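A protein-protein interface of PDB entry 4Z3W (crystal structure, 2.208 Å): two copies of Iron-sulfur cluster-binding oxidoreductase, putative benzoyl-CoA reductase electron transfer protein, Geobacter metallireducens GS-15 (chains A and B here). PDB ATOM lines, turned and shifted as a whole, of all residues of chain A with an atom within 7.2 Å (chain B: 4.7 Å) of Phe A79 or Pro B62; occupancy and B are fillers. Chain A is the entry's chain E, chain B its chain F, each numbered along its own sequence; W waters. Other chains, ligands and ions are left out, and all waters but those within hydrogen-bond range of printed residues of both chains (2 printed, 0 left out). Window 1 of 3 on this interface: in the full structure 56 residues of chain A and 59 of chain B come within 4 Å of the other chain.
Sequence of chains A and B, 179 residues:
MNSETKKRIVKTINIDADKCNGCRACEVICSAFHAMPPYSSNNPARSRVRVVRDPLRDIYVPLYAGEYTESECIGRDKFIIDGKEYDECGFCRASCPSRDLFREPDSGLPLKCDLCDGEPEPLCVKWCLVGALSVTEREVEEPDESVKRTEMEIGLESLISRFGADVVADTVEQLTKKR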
ATOM      1  N   ASP A  77      31.641  -0.395 -32.757  1.00  0.00           N
ATOM      2  CA  ASP A  77      30.578   0.452 -32.231  1.00  0.00           C
ATOM      3  C   ASP A  77      30.986   1.931 -32.157  1.00  0.00           C
ATOM      4  O   ASP A  77      32.162   2.260 -32.003  1.00  0.00           O
ATOM      5  CB  ASP A  77      30.107  -0.065 -30.858  1.00  0.00           C
ATOM      6  CG  ASP A  77      31.158   0.091 -29.749  1.00  0.00           C
ATOM      7  OD1 ASP A  77      32.344   0.354 -30.041  1.00  0.00           O
ATOM      8  OD2 ASP A  77      30.784  -0.080 -28.562  1.00  0.00           O
ATOM      9  N   LYS A  78      29.996   2.813 -32.292  1.00  0.00           N
ATOM     10  CA  LYS A  78      30.229   4.252 -32.284  1.00  0.00           C
ATOM     11  C   LYS A  78      29.080   5.033 -31.652  1.00  0.00           C
ATOM     12  O   LYS A  78      27.996   5.144 -32.230  1.00  0.00           O
ATOM     13  CB  LYS A  78      30.460   4.749 -33.704  1.00  0.00           C
ATOM     14  CG  LYS A  78      30.635   6.254 -33.816  1.00  0.00           C
ATOM     15  CD  LYS A  78      31.385   6.615 -35.089  1.00  0.00           C
ATOM     16  CE  LYS A  78      31.636   8.106 -35.179  1.00  0.00           C
ATOM     17  NZ  LYS A  78      30.349   8.870 -35.148  1.00  0.00           N
ATOM     18  N   PHE A  79      29.343   5.605 -30.477  1.00  0.00           N
ATOM     19  CA  PHE A  79      28.305   6.256 -29.680  1.00  0.00           C
ATOM     20  C   PHE A  79      28.124   7.759 -29.910  1.00  0.00           C
ATOM     21  O   PHE A  79      29.086   8.496 -30.108  1.00  0.00           O
ATOM     22  CB  PHE A  79      28.587   6.073 -28.188  1.00  0.00           C
ATOM     23  CG  PHE A  79      28.388   4.683 -27.688  1.00  0.00           C
ATOM     24  CD1 PHE A  79      27.108   4.194 -27.450  1.00  0.00           C
ATOM     25  CD2 PHE A  79      29.478   3.878 -27.413  1.00  0.00           C
ATOM     26  CE1 PHE A  79      26.915   2.916 -26.960  1.00  0.00           C
ATOM     27  CE2 PHE A  79      29.297   2.591 -26.936  1.00  0.00           C
ATOM     28  CZ  PHE A  79      28.008   2.112 -26.704  1.00  0.00           C
ATOM     29  N   ILE A  80      26.868   8.192 -29.849  1.00  0.00           N
ATOM     30  CA  ILE A  80      26.520   9.562 -29.515  1.00  0.00           C
ATOM     31  C   ILE A  80      25.939   9.531 -28.110  1.00  0.00           C
ATOM     32  O   ILE A  80      24.991   8.802 -27.850  1.00  0.00           O
ATOM     33  CB  ILE A  80      25.500  10.163 -30.483  1.00  0.00           C
ATOM     34  CG1 ILE A  80      26.086  10.239 -31.890  1.00  0.00           C
ATOM     35  CG2 ILE A  80      25.061  11.535 -29.995  1.00  0.00           C
ATOM     36  CD1 ILE A  80      25.117  10.781 -32.918  1.00  0.00           C
ATOM     37  N   ILE A  81      26.518  10.291 -27.189  1.00  0.00           N
ATOM     38  CA  ILE A  81      26.003  10.321 -25.817  1.00  0.00           C
ATOM     39  C   ILE A  81      26.010  11.743 -25.283  1.00  0.00           C
ATOM     40  O   ILE A  81      27.059  12.393 -25.269  1.00  0.00           O
ATOM     41  CB  ILE A  81      26.835   9.451 -24.852  1.00  0.00           C
ATOM     42  CG1 ILE A  81      27.015   8.038 -25.389  1.00  0.00           C
ATOM     43  CG2 ILE A  81      26.199   9.426 -23.470  1.00  0.00           C
ATOM     44  CD1 ILE A  81      28.083   7.261 -24.639  1.00  0.00           C
ATOM     45  N   LYS A  84      27.734  14.443 -27.458  1.00  0.00           N
ATOM     46  CA  LYS A  84      29.099  14.250 -27.927  1.00  0.00           C
ATOM     47  C   LYS A  84      29.172  13.052 -28.853  1.00  0.00           C
ATOM     48  O   LYS A  84      28.645  11.985 -28.542  1.00  0.00           O
ATOM     49  CB  LYS A  84      30.054  14.055 -26.750  1.00  0.00           C
ATOM     50  CG  LYS A  84      30.162  15.253 -25.827  1.00  0.00           C
ATOM     51  CD  LYS A  84      31.149  15.014 -24.692  1.00  0.00           C
ATOM     52  CE  LYS A  84      31.363  16.309 -23.906  1.00  0.00           C
ATOM     53  NZ  LYS A  84      32.140  16.102 -22.661  1.00  0.00           N
ATOM     54  N   GLU A  85      29.827  13.224 -29.993  1.00  0.00           N
ATOM     55  CA  GLU A  85      30.034  12.108 -30.910  1.00  0.00           C
ATOM     56  C   GLU A  85      31.399  11.479 -30.671  1.00  0.00           C
ATOM     57  O   GLU A  85      32.430  12.008 -31.102  1.00  0.00           O
ATOM     58  CB  GLU A  85      29.897  12.579 -32.350  1.00  0.00           C
ATOM     59  CG  GLU A  85      28.737  13.538 -32.517  1.00  0.00           C
ATOM     60  CD  GLU A  85      28.157  13.532 -33.916  1.00  0.00           C
ATOM     61  OE1 GLU A  85      28.496  12.620 -34.703  1.00  0.00           O
ATOM     62  OE2 GLU A  85      27.348  14.437 -34.219  1.00  0.00           O
ATOM     63  N   TYR A  86      31.409  10.355 -29.965  1.00  0.00           N
ATOM     64  CA  TYR A  86      32.667   9.704 -29.629  1.00  0.00           C
ATOM     65  C   TYR A  86      33.239   8.993 -30.842  1.00  0.00           C
ATOM     66  O   TYR A  86      32.579   8.896 -31.872  1.00  0.00           O
ATOM     67  CB  TYR A  86      32.469   8.738 -28.465  1.00  0.00           C
ATOM     68  CG  TYR A  86      32.200   9.480 -27.174  1.00  0.00           C
ATOM     69  CD1 TYR A  86      30.893   9.755 -26.750  1.00  0.00           C
ATOM     70  CD2 TYR A  86      33.250   9.949 -26.396  1.00  0.00           C
ATOM     71  CE1 TYR A  86      30.652  10.462 -25.572  1.00  0.00           C
ATOM     72  CE2 TYR A  86      33.018  10.650 -25.218  1.00  0.00           C
ATOM     73  CZ  TYR A  86      31.721  10.899 -24.813  1.00  0.00           C
ATOM     74  OH  TYR A  86      31.509  11.591 -23.651  1.00  0.00           O
ATOM     75  N   ASP A  87      34.482   8.533 -30.724  1.00  0.00           N
ATOM     76  CA  ASP A  87      35.137   7.795 -31.792  1.00  0.00           C
ATOM     77  C   ASP A  87      34.592   6.376 -31.915  1.00  0.00           C
ATOM     78  O   ASP A  87      34.079   5.795 -30.950  1.00  0.00           O
ATOM     79  CB  ASP A  87      36.644   7.720 -31.548  1.00  0.00           C
ATOM     80  CG  ASP A  87      37.291   9.085 -31.451  1.00  0.00           C
ATOM     81  OD1 ASP A  87      36.831  10.018 -32.146  1.00  0.00           O
ATOM     82  OD2 ASP A  87      38.263   9.210 -30.676  1.00  0.00           O
ATOM     83  N   GLU A  88      34.727   5.816 -33.106  1.00  0.00           N
ATOM     84  CA  GLU A  88      34.461   4.405 -33.309  1.00  0.00           C
ATOM     85  C   GLU A  88      35.364   3.614 -32.348  1.00  0.00           C
ATOM     86  O   GLU A  88      36.538   3.945 -32.200  1.00  0.00           O
ATOM     87  CB  GLU A  88      34.701   4.061 -34.781  1.00  0.00           C
ATOM     88  CG  GLU A  88      34.925   2.621 -35.120  1.00  0.00           C
ATOM     89  CD  GLU A  88      35.282   2.455 -36.578  1.00  0.00           C
ATOM     90  OE1 GLU A  88      36.485   2.361 -36.900  1.00  0.00           O
ATOM     91  OE2 GLU A  88      34.354   2.442 -37.410  1.00  0.00           O
ATOM     92  N   CYS A  89      34.814   2.609 -31.663  1.00  0.00           N
ATOM     93  CA  CYS A  89      35.581   1.860 -30.664  1.00  0.00           C
ATOM     94  C   CYS A  89      36.120   2.765 -29.563  1.00  0.00           C
ATOM     95  O   CYS A  89      37.153   2.469 -28.962  1.00  0.00           O
ATOM     96  CB  CYS A  89      36.748   1.123 -31.331  1.00  0.00           C
ATOM     97  SG  CYS A  89      36.248  -0.098 -32.592  1.00  0.00           S
ATOM     98  N   GLY A  90      35.413   3.862 -29.299  1.00  0.00           N
ATOM     99  CA  GLY A  90      35.903   4.918 -28.425  1.00  0.00           C
ATOM    100  C   GLY A  90      36.275   4.538 -27.004  1.00  0.00           C
ATOM    101  O   GLY A  90      37.186   5.125 -26.435  1.00  0.00           O
ATOM    102  N   PHE A  91      35.581   3.558 -26.433  1.00  0.00           N
ATOM    103  CA  PHE A  91      35.782   3.173 -25.036  1.00  0.00           C
ATOM    104  C   PHE A  91      36.419   1.804 -24.863  1.00  0.00           C
ATOM    105  O   PHE A  91      36.579   1.327 -23.753  1.00  0.00           O
ATOM    106  CB  PHE A  91      34.452   3.209 -24.294  1.00  0.00           C
ATOM    107  CG  PHE A  91      33.874   4.595 -24.170  1.00  0.00           C
ATOM    108  CD1 PHE A  91      34.291   5.444 -23.164  1.00  0.00           C
ATOM    109  CD2 PHE A  91      32.934   5.053 -25.076  1.00  0.00           C
ATOM    110  CE1 PHE A  91      33.765   6.720 -23.053  1.00  0.00           C
ATOM    111  CE2 PHE A  91      32.404   6.322 -24.968  1.00  0.00           C
ATOM    112  CZ  PHE A  91      32.820   7.159 -23.962  1.00  0.00           C
ATOM    113  N   ILE B  15      25.330   4.063 -32.627  1.00  0.00           N
ATOM    114  CA  ILE B  15      24.427   4.026 -31.494  1.00  0.00           C
ATOM    115  C   ILE B  15      24.194   5.430 -30.962  1.00  0.00           C
ATOM    116  O   ILE B  15      25.054   6.012 -30.291  1.00  0.00           O
ATOM    117  CB  ILE B  15      24.991   3.126 -30.387  1.00  0.00           C
ATOM    118  CG1 ILE B  15      25.288   1.738 -30.957  1.00  0.00           C
ATOM    119  CG2 ILE B  15      24.047   3.081 -29.197  1.00  0.00           C
ATOM    120  CD1 ILE B  15      25.881   0.737 -29.953  1.00  0.00           C
ATOM    121  N   ALA B  17      22.713   6.902 -28.325  1.00  0.00           N
ATOM    122  CA  ALA B  17      22.161   6.712 -26.978  1.00  0.00           C
ATOM    123  C   ALA B  17      21.262   7.869 -26.521  1.00  0.00           C
ATOM    124  O   ALA B  17      20.569   7.762 -25.502  1.00  0.00           O
ATOM    125  CB  ALA B  17      23.286   6.512 -25.979  1.00  0.00           C
ATOM    126  N   CYS B  20      17.705   6.567 -27.492  1.00  0.00           N
ATOM    127  CA  CYS B  20      17.233   5.295 -26.936  1.00  0.00           C
ATOM    128  C   CYS B  20      16.172   5.589 -25.900  1.00  0.00           C
ATOM    129  O   CYS B  20      16.219   6.627 -25.223  1.00  0.00           O
ATOM    130  CB  CYS B  20      18.381   4.482 -26.329  1.00  0.00           C
ATOM    131  SG  CYS B  20      17.869   2.928 -25.533  1.00  0.00           S
ATOM    132  N   VAL B  49      22.944  -7.925 -27.902  1.00  0.00           N
ATOM    133  CA  VAL B  49      22.877  -6.506 -27.593  1.00  0.00           C
ATOM    134  C   VAL B  49      22.188  -6.352 -26.239  1.00  0.00           C
ATOM    135  O   VAL B  49      21.110  -6.900 -26.018  1.00  0.00           O
ATOM    136  CB  VAL B  49      22.107  -5.708 -28.656  1.00  0.00           C
ATOM    137  CG1 VAL B  49      20.682  -6.252 -28.792  1.00  0.00           C
ATOM    138  CG2 VAL B  49      22.081  -4.231 -28.274  1.00  0.00           C
ATOM    139  N   ARG B  50      22.815  -5.614 -25.326  1.00  0.00           N
ATOM    140  CA  ARG B  50      22.275  -5.473 -23.985  1.00  0.00           C
ATOM    141  C   ARG B  50      22.287  -4.018 -23.561  1.00  0.00           C
ATOM    142  O   ARG B  50      23.322  -3.348 -23.627  1.00  0.00           O
ATOM    143  CB  ARG B  50      23.072  -6.322 -22.997  1.00  0.00           C
ATOM    144  CG  ARG B  50      23.077  -7.808 -23.315  1.00  0.00           C
ATOM    145  CD  ARG B  50      21.735  -8.463 -22.974  1.00  0.00           C
ATOM    146  NE  ARG B  50      21.338  -8.254 -21.586  1.00  0.00           N
ATOM    147  CZ  ARG B  50      21.664  -9.055 -20.577  1.00  0.00           C
ATOM    148  NH1 ARG B  50      22.409 -10.132 -20.778  1.00  0.00           N
ATOM    149  NH2 ARG B  50      21.244  -8.780 -19.354  1.00  0.00           N
ATOM    150  N   VAL B  51      21.135  -3.526 -23.126  1.00  0.00           N
ATOM    151  CA  VAL B  51      21.014  -2.118 -22.813  1.00  0.00           C
ATOM    152  C   VAL B  51      21.344  -1.794 -21.372  1.00  0.00           C
ATOM    153  O   VAL B  51      20.719  -2.308 -20.451  1.00  0.00           O
ATOM    154  CB  VAL B  51      19.611  -1.606 -23.095  1.00  0.00           C
ATOM    155  CG1 VAL B  51      19.608  -0.094 -23.008  1.00  0.00           C
ATOM    156  CG2 VAL B  51      19.145  -2.087 -24.464  1.00  0.00           C
ATOM    157  N   TYR B  60      20.851   5.337 -20.826  1.00  0.00           N
ATOM    158  CA  TYR B  60      20.297   4.359 -21.764  1.00  0.00           C
ATOM    159  C   TYR B  60      21.317   4.069 -22.845  1.00  0.00           C
ATOM    160  O   TYR B  60      21.416   4.818 -23.808  1.00  0.00           O
ATOM    161  CB  TYR B  60      19.020   4.880 -22.404  1.00  0.00           C
ATOM    162  CG  TYR B  60      18.031   5.389 -21.403  1.00  0.00           C
ATOM    163  CD1 TYR B  60      18.139   6.674 -20.895  1.00  0.00           C
ATOM    164  CD2 TYR B  60      16.990   4.581 -20.953  1.00  0.00           C
ATOM    165  CE1 TYR B  60      17.232   7.150 -19.969  1.00  0.00           C
ATOM    166  CE2 TYR B  60      16.076   5.042 -20.024  1.00  0.00           C
ATOM    167  CZ  TYR B  60      16.200   6.324 -19.532  1.00  0.00           C
ATOM    168  OH  TYR B  60      15.293   6.794 -18.602  1.00  0.00           O
ATOM    169  N   VAL B  61      22.056   2.971 -22.708  1.00  0.00           N
ATOM    170  CA  VAL B  61      23.186   2.724 -23.588  1.00  0.00           C
ATOM    171  C   VAL B  61      23.188   1.307 -24.173  1.00  0.00           C
ATOM    172  O   VAL B  61      23.555   0.361 -23.482  1.00  0.00           O
ATOM    173  CB  VAL B  61      24.504   2.958 -22.826  1.00  0.00           C
ATOM    174  CG1 VAL B  61      25.692   2.717 -23.727  1.00  0.00           C
ATOM    175  CG2 VAL B  61      24.537   4.372 -22.244  1.00  0.00           C
ATOM    176  N   PRO B  62      22.774   1.157 -25.451  1.00  0.00           N
ATOM    177  CA  PRO B  62      22.863  -0.165 -26.093  1.00  0.00           C
ATOM    178  C   PRO B  62      24.304  -0.652 -26.222  1.00  0.00           C
ATOM    179  O   PRO B  62      25.138   0.029 -26.811  1.00  0.00           O
ATOM    180  CB  PRO B  62      22.252   0.069 -27.476  1.00  0.00           C
ATOM    181  CG  PRO B  62      21.394   1.266 -27.324  1.00  0.00           C
ATOM    182  CD  PRO B  62      22.031   2.123 -26.273  1.00  0.00           C
ATOM    183  N   LEU B  63      24.596  -1.823 -25.675  1.00  0.00           N
ATOM    184  CA  LEU B  63      25.946  -2.360 -25.756  1.00  0.00           C
ATOM    185  C   LEU B  63      25.984  -3.653 -26.570  1.00  0.00           C
ATOM    186  O   LEU B  63      25.239  -4.598 -26.289  1.00  0.00           O
ATOM    187  CB  LEU B  63      26.491  -2.597 -24.356  1.00  0.00           C
ATOM    188  CG  LEU B  63      28.010  -2.601 -24.215  1.00  0.00           C
ATOM    189  CD1 LEU B  63      28.604  -1.317 -24.798  1.00  0.00           C
ATOM    190  CD2 LEU B  63      28.363  -2.729 -22.749  1.00  0.00           C
ATOM    191  N   TYR B  64      26.853  -3.701 -27.574  1.00  0.00           N
ATOM    192  CA  TYR B  64      26.937  -4.889 -28.415  1.00  0.00           C
ATOM    193  C   TYR B  64      28.079  -5.824 -28.023  1.00  0.00           C
ATOM    194  O   TYR B  64      29.208  -5.383 -27.789  1.00  0.00           O
ATOM    195  CB  TYR B  64      27.081  -4.479 -29.866  1.00  0.00           C
ATOM    196  CG  TYR B  64      25.800  -3.970 -30.478  1.00  0.00           C
ATOM    197  CD1 TYR B  64      25.274  -2.746 -30.108  1.00  0.00           C
ATOM    198  CD2 TYR B  64      25.117  -4.720 -31.427  1.00  0.00           C
ATOM    199  CE1 TYR B  64      24.114  -2.271 -30.683  1.00  0.00           C
ATOM    200  CE2 TYR B  64      23.954  -4.255 -32.005  1.00  0.00           C
ATOM    201  CZ  TYR B  64      23.462  -3.026 -31.638  1.00  0.00           C
ATOM    202  OH  TYR B  64      22.305  -2.558 -32.220  1.00  0.00           O
ATOM    203  N   PHE B  91      31.121   0.084 -20.409  1.00  0.00           N
ATOM    204  CA  PHE B  91      31.168   0.249 -21.852  1.00  0.00           C
ATOM    205  C   PHE B  91      31.866  -0.922 -22.528  1.00  0.00           C
ATOM    206  O   PHE B  91      32.025  -0.932 -23.744  1.00  0.00           O
ATOM    207  CB  PHE B  91      31.890   1.559 -22.225  1.00  0.00           C
ATOM    208  CG  PHE B  91      31.130   2.794 -21.849  1.00  0.00           C
ATOM    209  CD1 PHE B  91      30.052   3.220 -22.607  1.00  0.00           C
ATOM    210  CD2 PHE B  91      31.490   3.536 -20.736  1.00  0.00           C
ATOM    211  CE1 PHE B  91      29.345   4.368 -22.250  1.00  0.00           C
ATOM    212  CE2 PHE B  91      30.780   4.670 -20.380  1.00  0.00           C
ATOM    213  CZ  PHE B  91      29.711   5.085 -21.136  1.00  0.00           C
ATOM    214  N   LEU B 133      19.527   3.003 -33.563  1.00  0.00           N
ATOM    215  CA  LEU B 133      20.580   2.146 -34.111  1.00  0.00           C
ATOM    216  C   LEU B 133      20.663   2.179 -35.625  1.00  0.00           C
ATOM    217  O   LEU B 133      19.657   2.353 -36.305  1.00  0.00           O
ATOM    218  CB  LEU B 133      20.363   0.704 -33.682  1.00  0.00           C
ATOM    219  CG  LEU B 133      19.922   0.384 -32.264  1.00  0.00           C
ATOM    220  CD1 LEU B 133      19.558  -1.091 -32.174  1.00  0.00           C
ATOM    221  CD2 LEU B 133      21.027   0.710 -31.293  1.00  0.00           C
HETATM  222  O   HOH W   1      28.231  -1.199 -28.403  1.00  0.00           O
HETATM  223  O   HOH W   2      31.708   0.255 -26.142  1.00  0.00           O
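Of the 13 printed residues of chain B, 6 touch a printed residue of chain A.
Of the 13 printed residues of chain A, 5 touch a printed residue of chain B.
Printed residues of chain A that touch a printed residue of chain B: Lys A78, Phe A79, Ile A80, Ile A81 and Phe A91.
Hydrophobic or aromatic side chains of chain A within 4 Å of the printed part of chain B: Phe A79, Ile A81 and Phe A91.
Among the printed residues, 9 pairs touch across the chains.
Phe B91 touches its own counterpart, Phe A91.
Position printed for both chains: 91.
Of the 9 pairs that touch across the chains among the printed residues, 1 has its exchanged pair printed and touching as well.
N of Arg B50 lies within hydrogen-bond range of O of Leu B63.
The backbone carbonyl oxygen (O) of Phe A79 is in hydrogen-bond range of the backbone NH (N) of Tyr A86, 3.0 Å away.
Water W2 bridges the side-chain carboxylate of Asp A77 (2.6 Å) and the backbone carbonyl oxygen of Phe B91 (2.7 Å).
Water W1 bridges the side-chain carboxylate (OD2) of Asp A77 (2.8 Å) and the backbone NH (N) of Tyr B64 (3.0 Å).
Pro B62 touches just one residue of chain A: Phe A79.
Printed residues of chain A within 4 Å of Val B61: Phe A79.
Of the printed residues of chain A, Leu B63 touches Phe A79.
Printed residues of chain B within 4 Å of Ile A80: Ile B15 (2.9 Å) and Ala B17 (3.0 Å).
Printed residues of chain B within 4 Å of Lys A78: Ile B15.
Printed residues of chain B within 4 Å of Phe A91: Phe B91.
Cys A89 touches none of the printed residues of chain B.
Leu B133 touches none of the printed residues of chain A.
Among the printed residues, merely in contact across the chains: Phe A79 with Ile B15, Phe A79 with Pro B62, Phe A79 with Val B61, Phe A91 with Phe B91, Ile A81 with Phe B91 and Phe A79 with Leu B63.
O of Ile A80 is in hydrogen-bond range of N of Ala B17.
The backbone NH (N) of Ile A80 sits at hydrogen-bond distance from the backbone carbonyl oxygen (O) of Ile B15 (2.9 Å).
The backbone carbonyl oxygen (O) of Lys A78 lies within hydrogen-bond range of the backbone NH (N) of Ile B15, 2.9 Å away.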
